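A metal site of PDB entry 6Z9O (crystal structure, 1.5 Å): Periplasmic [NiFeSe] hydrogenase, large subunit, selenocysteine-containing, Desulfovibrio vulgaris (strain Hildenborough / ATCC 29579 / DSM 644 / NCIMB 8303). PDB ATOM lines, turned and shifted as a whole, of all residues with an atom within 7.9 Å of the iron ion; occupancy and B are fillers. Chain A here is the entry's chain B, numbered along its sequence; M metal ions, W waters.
The side-chain amide oxygen of Gln 429 lies close to the side-chain carboxylate of Glu 45 (3.3 Å). The side-chain carboxylate of Glu 45 lies within hydrogen-bond range of the side-chain hydroxyl of Thr 292 (2.7 Å). The backbone carbonyl oxygen of Cys 481 lies within hydrogen-bond range of a ring nitrogen (ND1) of His 484 (2.8 Å).
Of the 20 residues printed, 3 come within 4 Å of the iron ion.
OE2 of Glu 45 is bound to the iron ion (2.2 Å). NE2 of His 484 is bound to the iron ion (2.2 Å). Water W2 is bound to the iron ion (2.2 Å). Water W3 is bound to the iron ion (2.2 Å). O of Ile 430 is bound to the iron ion (2.2 Å). The iron ion is bound by water W1 (2.3 Å). The iron ion has six donor atoms within binding distance.
Water W2 lies within hydrogen-bond range of the side-chain carboxylate (OE1) of Glu 271 (2.5 Å), the side-chain amide oxygen (OE1) of Gln 429 (2.7 Å) and the side-chain amino group (NZ) of Lys 306 (3.0 Å). Water W1 bridges the side-chain carboxylate of Glu 45 (2.6 Å) and the side-chain amino group of Lys 306 (3.1 Å).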
ATOM      1  N   GLU A  45      -1.586  13.608 -30.174  1.00  0.00           N
ATOM      2  CA  GLU A  45      -0.797  13.431 -28.962  1.00  0.00           C
ATOM      3  C   GLU A  45       0.676  13.176 -29.272  1.00  0.00           C
ATOM      4  O   GLU A  45       1.539  13.514 -28.448  1.00  0.00           O
ATOM      5  CB  GLU A  45      -1.411  12.301 -28.132  1.00  0.00           C
ATOM      6  CG  GLU A  45      -2.756  12.726 -27.534  1.00  0.00           C
ATOM      7  CD  GLU A  45      -3.733  11.591 -27.267  1.00  0.00           C
ATOM      8  OE1 GLU A  45      -3.654  10.536 -27.934  1.00  0.00           O
ATOM      9  OE2 GLU A  45      -4.619  11.779 -26.401  1.00  0.00           O
ATOM     10  N   GLU A 271      -7.708   4.569 -19.611  1.00  0.00           N
ATOM     11  CA  GLU A 271      -8.045   4.339 -21.005  1.00  0.00           C
ATOM     12  C   GLU A 271      -7.562   2.945 -21.410  1.00  0.00           C
ATOM     13  O   GLU A 271      -6.364   2.646 -21.322  1.00  0.00           O
ATOM     14  CB  GLU A 271      -7.445   5.410 -21.908  1.00  0.00           C
ATOM     15  CG  GLU A 271      -8.049   6.792 -21.704  1.00  0.00           C
ATOM     16  CD  GLU A 271      -7.608   7.751 -22.773  1.00  0.00           C
ATOM     17  OE1 GLU A 271      -6.508   8.325 -22.654  1.00  0.00           O
ATOM     18  OE2 GLU A 271      -8.362   7.922 -23.754  1.00  0.00           O
ATOM     19  N   PHE A 278      -4.487   0.307 -30.991  1.00  0.00           N
ATOM     20  CA  PHE A 278      -3.303   0.806 -30.318  1.00  0.00           C
ATOM     21  C   PHE A 278      -2.566  -0.363 -29.675  1.00  0.00           C
ATOM     22  O   PHE A 278      -3.153  -1.416 -29.413  1.00  0.00           O
ATOM     23  CB  PHE A 278      -3.649   1.867 -29.266  1.00  0.00           C
ATOM     24  CG  PHE A 278      -4.318   3.076 -29.854  1.00  0.00           C
ATOM     25  CD1 PHE A 278      -3.563   4.059 -30.452  1.00  0.00           C
ATOM     26  CD2 PHE A 278      -5.689   3.184 -29.854  1.00  0.00           C
ATOM     27  CE1 PHE A 278      -4.171   5.165 -31.025  1.00  0.00           C
ATOM     28  CE2 PHE A 278      -6.302   4.281 -30.425  1.00  0.00           C
ATOM     29  CZ  PHE A 278      -5.545   5.268 -31.009  1.00  0.00           C
ATOM     30  N   TYR A 287      -4.491   9.193 -17.733  1.00  0.00           N
ATOM     31  CA  TYR A 287      -4.037  10.158 -18.725  1.00  0.00           C
ATOM     32  C   TYR A 287      -2.680  10.764 -18.355  1.00  0.00           C
ATOM     33  O   TYR A 287      -1.909  11.147 -19.238  1.00  0.00           O
ATOM     34  CB  TYR A 287      -5.095  11.263 -18.909  1.00  0.00           C
ATOM     35  CG  TYR A 287      -5.461  11.966 -17.628  1.00  0.00           C
ATOM     36  CD1 TYR A 287      -4.716  13.045 -17.186  1.00  0.00           C
ATOM     37  CD2 TYR A 287      -6.526  11.528 -16.854  1.00  0.00           C
ATOM     38  CE1 TYR A 287      -5.026  13.673 -15.998  1.00  0.00           C
ATOM     39  CE2 TYR A 287      -6.844  12.158 -15.673  1.00  0.00           C
ATOM     40  CZ  TYR A 287      -6.087  13.227 -15.245  1.00  0.00           C
ATOM     41  OH  TYR A 287      -6.405  13.857 -14.064  1.00  0.00           O
ATOM     42  N   GLY A 290      -0.444   8.591 -20.021  1.00  0.00           N
ATOM     43  CA  GLY A 290      -1.013   8.106 -21.247  1.00  0.00           C
ATOM     44  C   GLY A 290       0.038   7.918 -22.325  1.00  0.00           C
ATOM     45  O   GLY A 290       1.080   8.574 -22.334  1.00  0.00           O
ATOM     46  N   LYS A 291      -0.237   6.990 -23.236  1.00  0.00           N
ATOM     47  CA  LYS A 291       0.610   6.719 -24.379  1.00  0.00           C
ATOM     48  C   LYS A 291      -0.259   6.445 -25.589  1.00  0.00           C
ATOM     49  O   LYS A 291      -1.329   5.837 -25.463  1.00  0.00           O
ATOM     50  CB  LYS A 291       1.513   5.499 -24.170  1.00  0.00           C
ATOM     51  CG  LYS A 291       2.469   5.582 -23.009  1.00  0.00           C
ATOM     52  CD  LYS A 291       3.419   4.399 -23.115  1.00  0.00           C
ATOM     53  CE  LYS A 291       4.438   4.383 -21.999  1.00  0.00           C
ATOM     54  NZ  LYS A 291       5.335   5.567 -22.062  1.00  0.00           N
ATOM     55  N   THR A 292       0.206   6.877 -26.756  1.00  0.00           N
ATOM     56  CA  THR A 292      -0.555   6.751 -27.992  1.00  0.00           C
ATOM     57  C   THR A 292       0.360   6.121 -29.048  1.00  0.00           C
ATOM     58  O   THR A 292       1.175   6.800 -29.660  1.00  0.00           O
ATOM     59  CB  THR A 292      -1.096   8.107 -28.418  1.00  0.00           C
ATOM     60  OG1 THR A 292      -1.844   8.641 -27.311  1.00  0.00           O
ATOM     61  CG2 THR A 292      -2.004   7.964 -29.630  1.00  0.00           C
ATOM     62  N   PHE A 304     -10.374   3.454 -33.690  1.00  0.00           N
ATOM     63  CA  PHE A 304      -9.283   4.322 -33.270  1.00  0.00           C
ATOM     64  C   PHE A 304      -9.614   5.117 -32.007  1.00  0.00           C
ATOM     65  O   PHE A 304      -8.786   5.903 -31.540  1.00  0.00           O
ATOM     66  CB  PHE A 304      -8.889   5.300 -34.388  1.00  0.00           C
ATOM     67  CG  PHE A 304      -8.135   4.665 -35.524  1.00  0.00           C
ATOM     68  CD1 PHE A 304      -6.879   4.132 -35.326  1.00  0.00           C
ATOM     69  CD2 PHE A 304      -8.675   4.629 -36.802  1.00  0.00           C
ATOM     70  CE1 PHE A 304      -6.182   3.552 -36.357  1.00  0.00           C
ATOM     71  CE2 PHE A 304      -7.980   4.046 -37.848  1.00  0.00           C
ATOM     72  CZ  PHE A 304      -6.731   3.512 -37.626  1.00  0.00           C
ATOM     73  N   LYS A 306      -9.973   5.150 -28.115  1.00  0.00           N
ATOM     74  CA  LYS A 306      -9.642   4.411 -26.900  1.00  0.00           C
ATOM     75  C   LYS A 306     -10.911   4.234 -26.054  1.00  0.00           C
ATOM     76  O   LYS A 306     -11.942   4.850 -26.316  1.00  0.00           O
ATOM     77  CB  LYS A 306      -8.573   5.140 -26.081  1.00  0.00           C
ATOM     78  CG  LYS A 306      -7.206   5.298 -26.752  1.00  0.00           C
ATOM     79  CD  LYS A 306      -6.238   6.054 -25.845  1.00  0.00           C
ATOM     80  CE  LYS A 306      -4.849   6.260 -26.472  1.00  0.00           C
ATOM     81  NZ  LYS A 306      -3.997   7.192 -25.654  1.00  0.00           N
ATOM     82  N   LEU A 415     -10.647  16.868 -20.980  1.00  0.00           N
ATOM     83  CA  LEU A 415      -9.439  17.233 -20.259  1.00  0.00           C
ATOM     84  C   LEU A 415      -8.238  17.122 -21.185  1.00  0.00           C
ATOM     85  O   LEU A 415      -8.193  16.258 -22.072  1.00  0.00           O
ATOM     86  CB  LEU A 415      -9.217  16.376 -18.995  1.00  0.00           C
ATOM     87  CG  LEU A 415      -8.801  14.927 -19.218  1.00  0.00           C
ATOM     88  CD1 LEU A 415      -7.277  14.763 -19.248  1.00  0.00           C
ATOM     89  CD2 LEU A 415      -9.419  14.054 -18.130  1.00  0.00           C
ATOM     90  N   TYR A 428       1.466  14.947 -24.124  1.00  0.00           N
ATOM     91  CA  TYR A 428       0.208  15.667 -24.188  1.00  0.00           C
ATOM     92  C   TYR A 428      -0.867  14.621 -24.410  1.00  0.00           C
ATOM     93  O   TYR A 428      -0.817  13.893 -25.410  1.00  0.00           O
ATOM     94  CB  TYR A 428       0.190  16.699 -25.307  1.00  0.00           C
ATOM     95  CG  TYR A 428      -0.796  17.833 -25.112  1.00  0.00           C
ATOM     96  CD1 TYR A 428      -2.163  17.646 -25.303  1.00  0.00           C
ATOM     97  CD2 TYR A 428      -0.358  19.094 -24.728  1.00  0.00           C
ATOM     98  CE1 TYR A 428      -3.059  18.690 -25.123  1.00  0.00           C
ATOM     99  CE2 TYR A 428      -1.237  20.140 -24.551  1.00  0.00           C
ATOM    100  CZ  TYR A 428      -2.594  19.925 -24.744  1.00  0.00           C
ATOM    101  OH  TYR A 428      -3.467  20.983 -24.555  1.00  0.00           O
ATOM    102  N   GLN A 429      -1.824  14.537 -23.496  1.00  0.00           N
ATOM    103  CA  GLN A 429      -2.859  13.516 -23.561  1.00  0.00           C
ATOM    104  C   GLN A 429      -4.222  14.187 -23.490  1.00  0.00           C
ATOM    105  O   GLN A 429      -4.454  15.090 -22.688  1.00  0.00           O
ATOM    106  CB  GLN A 429      -2.686  12.496 -22.429  1.00  0.00           C
ATOM    107  CG  GLN A 429      -1.530  11.528 -22.684  1.00  0.00           C
ATOM    108  CD  GLN A 429      -1.780  10.604 -23.862  1.00  0.00           C
ATOM    109  OE1 GLN A 429      -2.899  10.130 -24.059  1.00  0.00           O
ATOM    110  NE2 GLN A 429      -0.738  10.345 -24.646  1.00  0.00           N
ATOM    111  N   ILE A 430      -5.117  13.735 -24.365  1.00  0.00           N
ATOM    112  CA  ILE A 430      -6.455  14.306 -24.524  1.00  0.00           C
ATOM    113  C   ILE A 430      -7.479  13.224 -24.270  1.00  0.00           C
ATOM    114  O   ILE A 430      -7.397  12.117 -24.831  1.00  0.00           O
ATOM    115  CB  ILE A 430      -6.627  14.930 -25.926  1.00  0.00           C
ATOM    116  CG1 ILE A 430      -5.686  16.130 -26.063  1.00  0.00           C
ATOM    117  CG2 ILE A 430      -8.074  15.356 -26.133  1.00  0.00           C
ATOM    118  CD1 ILE A 430      -5.053  16.251 -27.410  1.00  0.00           C
ATOM    119  N   VAL A 431      -8.444  13.525 -23.411  1.00  0.00           N
ATOM    120  CA  VAL A 431      -9.548  12.646 -23.052  1.00  0.00           C
ATOM    121  C   VAL A 431     -10.781  13.514 -23.277  1.00  0.00           C
ATOM    122  O   VAL A 431     -11.075  14.401 -22.470  1.00  0.00           O
ATOM    123  CB  VAL A 431      -9.464  12.132 -21.605  1.00  0.00           C
ATOM    124  CG1 VAL A 431     -10.621  11.193 -21.263  1.00  0.00           C
ATOM    125  CG2 VAL A 431      -8.138  11.446 -21.353  1.00  0.00           C
ATOM    126  N   SER A 432     -11.488  13.277 -24.371  1.00  0.00           N
ATOM    127  CA  SER A 432     -12.467  14.205 -24.892  1.00  0.00           C
ATOM    128  C   SER A 432     -13.899  13.672 -24.727  1.00  0.00           C
ATOM    129  O   SER A 432     -14.129  12.538 -24.290  1.00  0.00           O
ATOM    130  CB  SER A 432     -12.166  14.491 -26.362  1.00  0.00           C
ATOM    131  OG  SER A 432     -12.296  13.294 -27.101  1.00  0.00           O
ATOM    132  N   LEU A 435     -15.095  10.803 -27.040  1.00  0.00           N
ATOM    133  CA  LEU A 435     -14.374   9.629 -26.562  1.00  0.00           C
ATOM    134  C   LEU A 435     -15.199   8.884 -25.518  1.00  0.00           C
ATOM    135  O   LEU A 435     -15.353   7.661 -25.591  1.00  0.00           O
ATOM    136  CB  LEU A 435     -13.026  10.049 -25.982  1.00  0.00           C
ATOM    137  CG  LEU A 435     -12.235   9.017 -25.172  1.00  0.00           C
ATOM    138  CD1 LEU A 435     -11.530   8.030 -26.062  1.00  0.00           C
ATOM    139  CD2 LEU A 435     -11.244   9.723 -24.242  1.00  0.00           C
ATOM    140  N   CYS A 481     -12.991  14.560 -32.491  1.00  0.00           N
ATOM    141  CA  CYS A 481     -12.675  14.727 -31.073  1.00  0.00           C
ATOM    142  C   CYS A 481     -12.387  13.397 -30.407  1.00  0.00           C
ATOM    143  O   CYS A 481     -11.501  13.300 -29.554  1.00  0.00           O
ATOM    144  CB  CYS A 481     -13.830  15.398 -30.343  1.00  0.00           C
ATOM    145  SG  CYS A 481     -13.862  17.156 -30.489  1.00  0.00           S
ATOM    146  N   ALA A 482     -13.164  12.362 -30.744  1.00  0.00           N
ATOM    147  CA  ALA A 482     -13.047  11.099 -30.041  1.00  0.00           C
ATOM    148  C   ALA A 482     -11.683  10.458 -30.286  1.00  0.00           C
ATOM    149  O   ALA A 482     -11.132   9.826 -29.379  1.00  0.00           O
ATOM    150  CB  ALA A 482     -14.167  10.153 -30.461  1.00  0.00           C
ATOM    151  N   VAL A 483     -11.124  10.611 -31.484  1.00  0.00           N
ATOM    152  CA  VAL A 483      -9.877   9.948 -31.877  1.00  0.00           C
ATOM    153  C   VAL A 483      -8.678  10.879 -31.741  1.00  0.00           C
ATOM    154  O   VAL A 483      -7.623  10.481 -31.232  1.00  0.00           O
ATOM    155  CB  VAL A 483      -9.987   9.406 -33.320  1.00  0.00           C
ATOM    156  CG1 VAL A 483      -8.662   8.759 -33.733  1.00  0.00           C
ATOM    157  CG2 VAL A 483     -11.151   8.429 -33.442  1.00  0.00           C
ATOM    158  N   HIS A 484      -8.811  12.110 -32.223  1.00  0.00           N
ATOM    159  CA  HIS A 484      -7.726  13.095 -32.281  1.00  0.00           C
ATOM    160  C   HIS A 484      -6.433  12.437 -32.784  1.00  0.00           C
ATOM    161  O   HIS A 484      -6.463  11.720 -33.796  1.00  0.00           O
ATOM    162  CB  HIS A 484      -7.522  13.809 -30.919  1.00  0.00           C
ATOM    163  CG  HIS A 484      -7.636  12.937 -29.694  1.00  0.00           C
ATOM    164  ND1 HIS A 484      -8.843  12.594 -29.134  1.00  0.00           N
ATOM    165  CD2 HIS A 484      -6.681  12.406 -28.893  1.00  0.00           C
ATOM    166  CE1 HIS A 484      -8.635  11.850 -28.054  1.00  0.00           C
ATOM    167  NE2 HIS A 484      -7.329  11.726 -27.895  1.00  0.00           N
ATOM    168  OXT HIS A 484      -5.340  12.633 -32.244  1.00  0.00           O
HETATM  169 FE    FE M   1      -6.466  10.660 -26.210  1.00  0.00          FE
HETATM  170  O   HOH W   1      -5.688   9.006 -27.569  1.00  0.00           O
HETATM  171  O   HOH W   2      -5.446   9.597 -24.577  1.00  0.00           O
HETATM  172  O   HOH W   3      -8.246   9.405 -25.867  1.00  0.00           O
